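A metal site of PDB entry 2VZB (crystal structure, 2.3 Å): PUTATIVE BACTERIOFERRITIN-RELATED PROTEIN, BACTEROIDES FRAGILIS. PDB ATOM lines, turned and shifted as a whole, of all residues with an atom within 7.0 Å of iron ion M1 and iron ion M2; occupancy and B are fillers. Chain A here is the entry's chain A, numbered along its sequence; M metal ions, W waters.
The side-chain hydroxyl (OH) of Tyr 121 lies close to the side-chain carboxylate (OE2) of Glu 29 (2.5 Å). The side-chain hydroxyl (OH) of Tyr 36 lies close to the side-chain carboxylate (OE2) of Glu 114. A ring nitrogen (NE2) of His 149 sits at hydrogen-bond distance from the side-chain carboxylate (OE1) of Glu 61, 2.7 Å away. OE1 of Glu 145 sits at hydrogen-bond distance from NE2 of His 65, 2.7 Å away. NE2 of His 65 lies close to O of Glu 61 (3.4 Å).
The nearest printed residue that does not touch iron ion M1 is Tyr 36 (4.4 Å).
The nearest printed residue that does not touch iron ion M2 is Ile 142 (4.2 Å).
Iron ion M1 is bound by OE1 of Glu 146 (2.1 Å), OE2 of Glu 62 (2.1 Å), OE1 of Glu 114 (2.2 Å), ND1 of His 149 (2.3 Å), water W1 (2.3 Å) and OE2 of Glu 114 (2.5 Å).
OE1 of Glu 62 binds iron ion M2 (2.0 Å). The side-chain carboxylate (OE2) of Glu 146 is bound to iron ion M2 (2.1 Å). OE1 of Glu 29 binds iron ion M2 (2.2 Å). Iron ion M2 is bound by the side-chain carboxylate (OE2) of Glu 29 (2.2 Å). Iron ion M2 is bound by a ring nitrogen (ND1) of His 65 (2.3 Å). Water W2 binds iron ion M2, 2.5 Å away.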
ATOM      1  N   ALA A  25     -24.621  22.352 -13.169  1.00  0.00           N
ATOM      2  CA  ALA A  25     -25.308  22.050 -14.454  1.00  0.00           C
ATOM      3  C   ALA A  25     -24.317  21.976 -15.640  1.00  0.00           C
ATOM      4  O   ALA A  25     -24.363  21.048 -16.451  1.00  0.00           O
ATOM      5  CB  ALA A  25     -26.359  23.074 -14.718  1.00  0.00           C
ATOM      6  N   GLU A  28     -22.276  18.936 -15.563  1.00  0.00           N
ATOM      7  CA  GLU A  28     -23.152  17.819 -15.964  1.00  0.00           C
ATOM      8  C   GLU A  28     -23.377  17.733 -17.473  1.00  0.00           C
ATOM      9  O   GLU A  28     -23.431  16.643 -18.030  1.00  0.00           O
ATOM     10  CB  GLU A  28     -24.493  17.938 -15.219  1.00  0.00           C
ATOM     11  CG  GLU A  28     -24.354  17.609 -13.758  1.00  0.00           C
ATOM     12  CD  GLU A  28     -25.501  18.077 -12.919  1.00  0.00           C
ATOM     13  OE1 GLU A  28     -26.404  18.739 -13.472  1.00  0.00           O
ATOM     14  OE2 GLU A  28     -25.510  17.769 -11.712  1.00  0.00           O
ATOM     15  N   GLU A  29     -23.532  18.893 -18.116  1.00  0.00           N
ATOM     16  CA  GLU A  29     -23.737  18.967 -19.572  1.00  0.00           C
ATOM     17  C   GLU A  29     -22.530  18.383 -20.308  1.00  0.00           C
ATOM     18  O   GLU A  29     -22.678  17.587 -21.215  1.00  0.00           O
ATOM     19  CB  GLU A  29     -24.016  20.408 -20.033  1.00  0.00           C
ATOM     20  CG  GLU A  29     -25.392  20.944 -19.596  1.00  0.00           C
ATOM     21  CD  GLU A  29     -26.543  20.206 -20.256  1.00  0.00           C
ATOM     22  OE1 GLU A  29     -26.319  19.513 -21.285  1.00  0.00           O
ATOM     23  OE2 GLU A  29     -27.693  20.314 -19.751  1.00  0.00           O
ATOM     24  N   ALA A  32     -22.569  14.605 -19.825  1.00  0.00           N
ATOM     25  CA  ALA A  32     -23.652  14.075 -20.656  1.00  0.00           C
ATOM     26  C   ALA A  32     -23.313  14.116 -22.150  1.00  0.00           C
ATOM     27  O   ALA A  32     -23.542  13.161 -22.882  1.00  0.00           O
ATOM     28  CB  ALA A  32     -24.945  14.825 -20.372  1.00  0.00           C
ATOM     29  N   TYR A  33     -22.714  15.221 -22.560  1.00  0.00           N
ATOM     30  CA  TYR A  33     -22.212  15.417 -23.935  1.00  0.00           C
ATOM     31  C   TYR A  33     -21.233  14.318 -24.325  1.00  0.00           C
ATOM     32  O   TYR A  33     -21.426  13.625 -25.332  1.00  0.00           O
ATOM     33  CB  TYR A  33     -21.573  16.830 -24.016  1.00  0.00           C
ATOM     34  CG  TYR A  33     -20.827  17.225 -25.271  1.00  0.00           C
ATOM     35  CD1 TYR A  33     -21.144  16.720 -26.519  1.00  0.00           C
ATOM     36  CD2 TYR A  33     -19.850  18.209 -25.188  1.00  0.00           C
ATOM     37  CE1 TYR A  33     -20.444  17.133 -27.646  1.00  0.00           C
ATOM     38  CE2 TYR A  33     -19.165  18.625 -26.298  1.00  0.00           C
ATOM     39  CZ  TYR A  33     -19.470  18.081 -27.516  1.00  0.00           C
ATOM     40  OH  TYR A  33     -18.769  18.538 -28.599  1.00  0.00           O
ATOM     41  N   TYR A  36     -22.845  10.685 -24.407  1.00  0.00           N
ATOM     42  CA  TYR A  36     -23.552  10.438 -25.689  1.00  0.00           C
ATOM     43  C   TYR A  36     -22.584  10.251 -26.865  1.00  0.00           C
ATOM     44  O   TYR A  36     -22.773   9.393 -27.726  1.00  0.00           O
ATOM     45  CB  TYR A  36     -24.462  11.603 -26.005  1.00  0.00           C
ATOM     46  CG  TYR A  36     -25.858  11.494 -25.467  1.00  0.00           C
ATOM     47  CD1 TYR A  36     -26.664  10.387 -25.734  1.00  0.00           C
ATOM     48  CD2 TYR A  36     -26.407  12.521 -24.718  1.00  0.00           C
ATOM     49  CE1 TYR A  36     -27.982  10.313 -25.266  1.00  0.00           C
ATOM     50  CE2 TYR A  36     -27.719  12.454 -24.246  1.00  0.00           C
ATOM     51  CZ  TYR A  36     -28.481  11.347 -24.525  1.00  0.00           C
ATOM     52  OH  TYR A  36     -29.755  11.302 -24.020  1.00  0.00           O
ATOM     53  N   HIS A  58     -28.178  14.081 -29.699  1.00  0.00           N
ATOM     54  CA  HIS A  58     -28.242  14.470 -28.291  1.00  0.00           C
ATOM     55  C   HIS A  58     -26.919  15.037 -27.779  1.00  0.00           C
ATOM     56  O   HIS A  58     -26.900  16.021 -27.036  1.00  0.00           O
ATOM     57  CB  HIS A  58     -28.731  13.297 -27.441  1.00  0.00           C
ATOM     58  CG  HIS A  58     -30.167  12.963 -27.675  1.00  0.00           C
ATOM     59  ND1 HIS A  58     -30.903  12.174 -26.812  1.00  0.00           N
ATOM     60  CD2 HIS A  58     -31.030  13.347 -28.649  1.00  0.00           C
ATOM     61  CE1 HIS A  58     -32.134  12.059 -27.276  1.00  0.00           C
ATOM     62  NE2 HIS A  58     -32.240  12.770 -28.384  1.00  0.00           N
ATOM     63  N   GLU A  61     -26.967  18.512 -28.858  1.00  0.00           N
ATOM     64  CA  GLU A  61     -27.919  19.291 -28.053  1.00  0.00           C
ATOM     65  C   GLU A  61     -27.417  19.623 -26.645  1.00  0.00           C
ATOM     66  O   GLU A  61     -27.600  20.731 -26.170  1.00  0.00           O
ATOM     67  CB  GLU A  61     -29.294  18.610 -28.042  1.00  0.00           C
ATOM     68  CG  GLU A  61     -29.954  18.746 -29.435  1.00  0.00           C
ATOM     69  CD  GLU A  61     -31.256  18.000 -29.605  1.00  0.00           C
ATOM     70  OE1 GLU A  61     -31.549  17.042 -28.867  1.00  0.00           O
ATOM     71  OE2 GLU A  61     -31.992  18.387 -30.532  1.00  0.00           O
ATOM     72  N   GLU A  62     -26.743  18.673 -26.001  1.00  0.00           N
ATOM     73  CA  GLU A  62     -26.129  18.952 -24.676  1.00  0.00           C
ATOM     74  C   GLU A  62     -25.009  19.953 -24.815  1.00  0.00           C
ATOM     75  O   GLU A  62     -24.834  20.805 -23.972  1.00  0.00           O
ATOM     76  CB  GLU A  62     -25.533  17.699 -23.997  1.00  0.00           C
ATOM     77  CG  GLU A  62     -26.372  16.452 -23.994  1.00  0.00           C
ATOM     78  CD  GLU A  62     -27.722  16.631 -23.320  1.00  0.00           C
ATOM     79  OE1 GLU A  62     -28.100  17.732 -22.912  1.00  0.00           O
ATOM     80  OE2 GLU A  62     -28.427  15.614 -23.196  1.00  0.00           O
ATOM     81  N   ARG A  63     -24.220  19.803 -25.863  1.00  0.00           N
ATOM     82  CA  ARG A  63     -23.179  20.780 -26.199  1.00  0.00           C
ATOM     83  C   ARG A  63     -23.721  22.204 -26.247  1.00  0.00           C
ATOM     84  O   ARG A  63     -23.078  23.104 -25.707  1.00  0.00           O
ATOM     85  CB  ARG A  63     -22.548  20.416 -27.533  1.00  0.00           C
ATOM     86  CG  ARG A  63     -21.443  21.364 -28.003  1.00  0.00           C
ATOM     87  CD  ARG A  63     -20.395  21.706 -26.960  1.00  0.00           C
ATOM     88  NE  ARG A  63     -19.439  22.653 -27.543  1.00  0.00           N
ATOM     89  CZ  ARG A  63     -19.589  23.980 -27.532  1.00  0.00           C
ATOM     90  NH1 ARG A  63     -20.636  24.563 -26.936  1.00  0.00           N
ATOM     91  NH2 ARG A  63     -18.656  24.716 -28.126  1.00  0.00           N
ATOM     92  N   HIS A  65     -26.581  23.223 -24.786  1.00  0.00           N
ATOM     93  CA  HIS A  65     -27.014  23.518 -23.399  1.00  0.00           C
ATOM     94  C   HIS A  65     -25.876  24.117 -22.595  1.00  0.00           C
ATOM     95  O   HIS A  65     -26.039  25.115 -21.899  1.00  0.00           O
ATOM     96  CB  HIS A  65     -27.479  22.264 -22.656  1.00  0.00           C
ATOM     97  CG  HIS A  65     -28.697  21.627 -23.236  1.00  0.00           C
ATOM     98  ND1 HIS A  65     -29.094  20.363 -22.889  1.00  0.00           N
ATOM     99  CD2 HIS A  65     -29.574  22.069 -24.170  1.00  0.00           C
ATOM    100  CE1 HIS A  65     -30.185  20.048 -23.577  1.00  0.00           C
ATOM    101  NE2 HIS A  65     -30.501  21.064 -24.358  1.00  0.00           N
ATOM    102  N   ALA A  66     -24.707  23.496 -22.696  1.00  0.00           N
ATOM    103  CA  ALA A  66     -23.475  23.971 -22.044  1.00  0.00           C
ATOM    104  C   ALA A  66     -23.183  25.448 -22.360  1.00  0.00           C
ATOM    105  O   ALA A  66     -22.827  26.229 -21.461  1.00  0.00           O
ATOM    106  CB  ALA A  66     -22.283  23.108 -22.432  1.00  0.00           C
ATOM    107  N   ILE A  69     -25.694  27.854 -20.760  1.00  0.00           N
ATOM    108  CA  ILE A  69     -25.424  27.950 -19.329  1.00  0.00           C
ATOM    109  C   ILE A  69     -24.182  28.791 -19.076  1.00  0.00           C
ATOM    110  O   ILE A  69     -24.205  29.737 -18.304  1.00  0.00           O
ATOM    111  CB  ILE A  69     -25.252  26.549 -18.695  1.00  0.00           C
ATOM    112  CG1 ILE A  69     -26.590  25.815 -18.689  1.00  0.00           C
ATOM    113  CG2 ILE A  69     -24.678  26.653 -17.246  1.00  0.00           C
ATOM    114  CD1 ILE A  69     -26.424  24.292 -18.544  1.00  0.00           C
ATOM    115  N   ASN A 110     -28.167   6.343 -20.446  1.00  0.00           N
ATOM    116  CA  ASN A 110     -28.477   7.711 -20.881  1.00  0.00           C
ATOM    117  C   ASN A 110     -29.842   8.193 -20.362  1.00  0.00           C
ATOM    118  O   ASN A 110     -29.992   9.361 -20.015  1.00  0.00           O
ATOM    119  CB  ASN A 110     -28.304   7.855 -22.384  1.00  0.00           C
ATOM    120  CG  ASN A 110     -26.854   7.865 -22.793  1.00  0.00           C
ATOM    121  OD1 ASN A 110     -26.096   8.710 -22.358  1.00  0.00           O
ATOM    122  ND2 ASN A 110     -26.454   6.900 -23.598  1.00  0.00           N
ATOM    123  N   SER A 113     -29.149   9.545 -16.882  1.00  0.00           N
ATOM    124  CA  SER A 113     -28.506  10.832 -16.988  1.00  0.00           C
ATOM    125  C   SER A 113     -29.537  11.895 -17.301  1.00  0.00           C
ATOM    126  O   SER A 113     -29.497  12.974 -16.730  1.00  0.00           O
ATOM    127  CB  SER A 113     -27.420  10.780 -18.047  1.00  0.00           C
ATOM    128  OG  SER A 113     -26.533   9.713 -17.778  1.00  0.00           O
ATOM    129  N   GLU A 114     -30.464  11.571 -18.219  1.00  0.00           N
ATOM    130  CA  GLU A 114     -31.570  12.464 -18.569  1.00  0.00           C
ATOM    131  C   GLU A 114     -32.460  12.828 -17.399  1.00  0.00           C
ATOM    132  O   GLU A 114     -32.787  13.982 -17.204  1.00  0.00           O
ATOM    133  CB  GLU A 114     -32.461  11.855 -19.665  1.00  0.00           C
ATOM    134  CG  GLU A 114     -31.814  11.748 -21.015  1.00  0.00           C
ATOM    135  CD  GLU A 114     -31.229  13.043 -21.549  1.00  0.00           C
ATOM    136  OE1 GLU A 114     -31.752  14.139 -21.232  1.00  0.00           O
ATOM    137  OE2 GLU A 114     -30.246  12.947 -22.318  1.00  0.00           O
ATOM    138  N   ALA A 117     -30.833  15.206 -15.280  1.00  0.00           N
ATOM    139  CA  ALA A 117     -30.855  16.523 -15.941  1.00  0.00           C
ATOM    140  C   ALA A 117     -32.208  17.219 -15.774  1.00  0.00           C
ATOM    141  O   ALA A 117     -32.269  18.406 -15.483  1.00  0.00           O
ATOM    142  CB  ALA A 117     -30.488  16.386 -17.425  1.00  0.00           C
ATOM    143  N   TYR A 121     -32.859  21.051 -13.940  1.00  0.00           N
ATOM    144  CA  TYR A 121     -33.444  22.236 -14.584  1.00  0.00           C
ATOM    145  C   TYR A 121     -34.770  22.627 -13.954  1.00  0.00           C
ATOM    146  O   TYR A 121     -35.102  23.814 -13.889  1.00  0.00           O
ATOM    147  CB  TYR A 121     -33.459  22.131 -16.125  1.00  0.00           C
ATOM    148  CG  TYR A 121     -32.034  22.003 -16.598  1.00  0.00           C
ATOM    149  CD1 TYR A 121     -31.118  23.042 -16.407  1.00  0.00           C
ATOM    150  CD2 TYR A 121     -31.562  20.823 -17.113  1.00  0.00           C
ATOM    151  CE1 TYR A 121     -29.816  22.918 -16.768  1.00  0.00           C
ATOM    152  CE2 TYR A 121     -30.241  20.686 -17.478  1.00  0.00           C
ATOM    153  CZ  TYR A 121     -29.369  21.736 -17.295  1.00  0.00           C
ATOM    154  OH  TYR A 121     -28.046  21.615 -17.667  1.00  0.00           O
ATOM    155  N   ILE A 142     -33.910  24.276 -21.756  1.00  0.00           N
ATOM    156  CA  ILE A 142     -33.087  23.074 -21.600  1.00  0.00           C
ATOM    157  C   ILE A 142     -33.946  21.926 -21.082  1.00  0.00           C
ATOM    158  O   ILE A 142     -33.953  20.842 -21.639  1.00  0.00           O
ATOM    159  CB  ILE A 142     -31.873  23.324 -20.667  1.00  0.00           C
ATOM    160  CG1 ILE A 142     -30.997  24.441 -21.251  1.00  0.00           C
ATOM    161  CG2 ILE A 142     -31.053  22.042 -20.463  1.00  0.00           C
ATOM    162  CD1 ILE A 142     -29.768  24.786 -20.460  1.00  0.00           C
ATOM    163  N   GLU A 145     -36.041  20.186 -23.661  1.00  0.00           N
ATOM    164  CA  GLU A 145     -35.189  19.299 -24.456  1.00  0.00           C
ATOM    165  C   GLU A 145     -34.830  17.998 -23.715  1.00  0.00           C
ATOM    166  O   GLU A 145     -34.813  16.926 -24.326  1.00  0.00           O
ATOM    167  CB  GLU A 145     -33.923  20.020 -24.956  1.00  0.00           C
ATOM    168  CG  GLU A 145     -34.266  21.197 -25.917  1.00  0.00           C
ATOM    169  CD  GLU A 145     -33.126  21.612 -26.830  1.00  0.00           C
ATOM    170  OE1 GLU A 145     -31.964  21.259 -26.564  1.00  0.00           O
ATOM    171  OE2 GLU A 145     -33.436  22.316 -27.820  1.00  0.00           O
ATOM    172  N   GLU A 146     -34.550  18.096 -22.424  1.00  0.00           N
ATOM    173  CA  GLU A 146     -34.180  16.898 -21.636  1.00  0.00           C
ATOM    174  C   GLU A 146     -35.359  15.925 -21.540  1.00  0.00           C
ATOM    175  O   GLU A 146     -35.168  14.714 -21.619  1.00  0.00           O
ATOM    176  CB  GLU A 146     -33.685  17.236 -20.229  1.00  0.00           C
ATOM    177  CG  GLU A 146     -32.654  18.386 -20.097  1.00  0.00           C
ATOM    178  CD  GLU A 146     -31.331  18.082 -20.732  1.00  0.00           C
ATOM    179  OE1 GLU A 146     -31.241  17.106 -21.491  1.00  0.00           O
ATOM    180  OE2 GLU A 146     -30.366  18.820 -20.460  1.00  0.00           O
ATOM    181  N   GLU A 147     -36.565  16.462 -21.384  1.00  0.00           N
ATOM    182  CA  GLU A 147     -37.780  15.645 -21.396  1.00  0.00           C
ATOM    183  C   GLU A 147     -37.972  14.946 -22.740  1.00  0.00           C
ATOM    184  O   GLU A 147     -38.432  13.799 -22.789  1.00  0.00           O
ATOM    185  CB  GLU A 147     -39.019  16.493 -21.089  1.00  0.00           C
ATOM    186  CG  GLU A 147     -39.041  17.091 -19.696  1.00  0.00           C
ATOM    187  CD  GLU A 147     -40.386  17.686 -19.334  1.00  0.00           C
ATOM    188  OE1 GLU A 147     -41.395  16.971 -19.364  1.00  0.00           O
ATOM    189  OE2 GLU A 147     -40.453  18.881 -19.000  1.00  0.00           O
ATOM    190  N   HIS A 149     -35.472  14.213 -24.865  1.00  0.00           N
ATOM    191  CA  HIS A 149     -34.395  13.213 -24.875  1.00  0.00           C
ATOM    192  C   HIS A 149     -34.821  11.952 -24.149  1.00  0.00           C
ATOM    193  O   HIS A 149     -34.589  10.846 -24.646  1.00  0.00           O
ATOM    194  CB  HIS A 149     -33.132  13.712 -24.159  1.00  0.00           C
ATOM    195  CG  HIS A 149     -32.369  14.760 -24.910  1.00  0.00           C
ATOM    196  ND1 HIS A 149     -31.314  15.442 -24.339  1.00  0.00           N
ATOM    197  CD2 HIS A 149     -32.522  15.257 -26.162  1.00  0.00           C
ATOM    198  CE1 HIS A 149     -30.841  16.300 -25.218  1.00  0.00           C
ATOM    199  NE2 HIS A 149     -31.545  16.199 -26.322  1.00  0.00           N
ATOM    200  N   GLU A 150     -35.387  12.116 -22.962  1.00  0.00           N
ATOM    201  CA  GLU A 150     -35.888  10.968 -22.191  1.00  0.00           C
ATOM    202  C   GLU A 150     -36.879  10.161 -23.016  1.00  0.00           C
ATOM    203  O   GLU A 150     -36.737   8.943 -23.141  1.00  0.00           O
ATOM    204  CB  GLU A 150     -36.562  11.362 -20.849  1.00  0.00           C
ATOM    205  CG  GLU A 150     -36.655  10.144 -19.939  1.00  0.00           C
ATOM    206  CD  GLU A 150     -37.797  10.167 -18.923  1.00  0.00           C
ATOM    207  OE1 GLU A 150     -38.372  11.250 -18.610  1.00  0.00           O
ATOM    208  OE2 GLU A 150     -38.089   9.050 -18.419  1.00  0.00           O
HETATM  209 FE    FE M   1     -30.334  15.451 -22.311  1.00  0.00          FE
HETATM  210 FE    FE M   2     -28.409  18.896 -21.307  1.00  0.00          FE
HETATM  211  O   HOH W   1     -29.248  15.029 -20.291  1.00  0.00           O
HETATM  212  O   HOH W   2     -27.412  16.983 -20.036  1.00  0.00           O
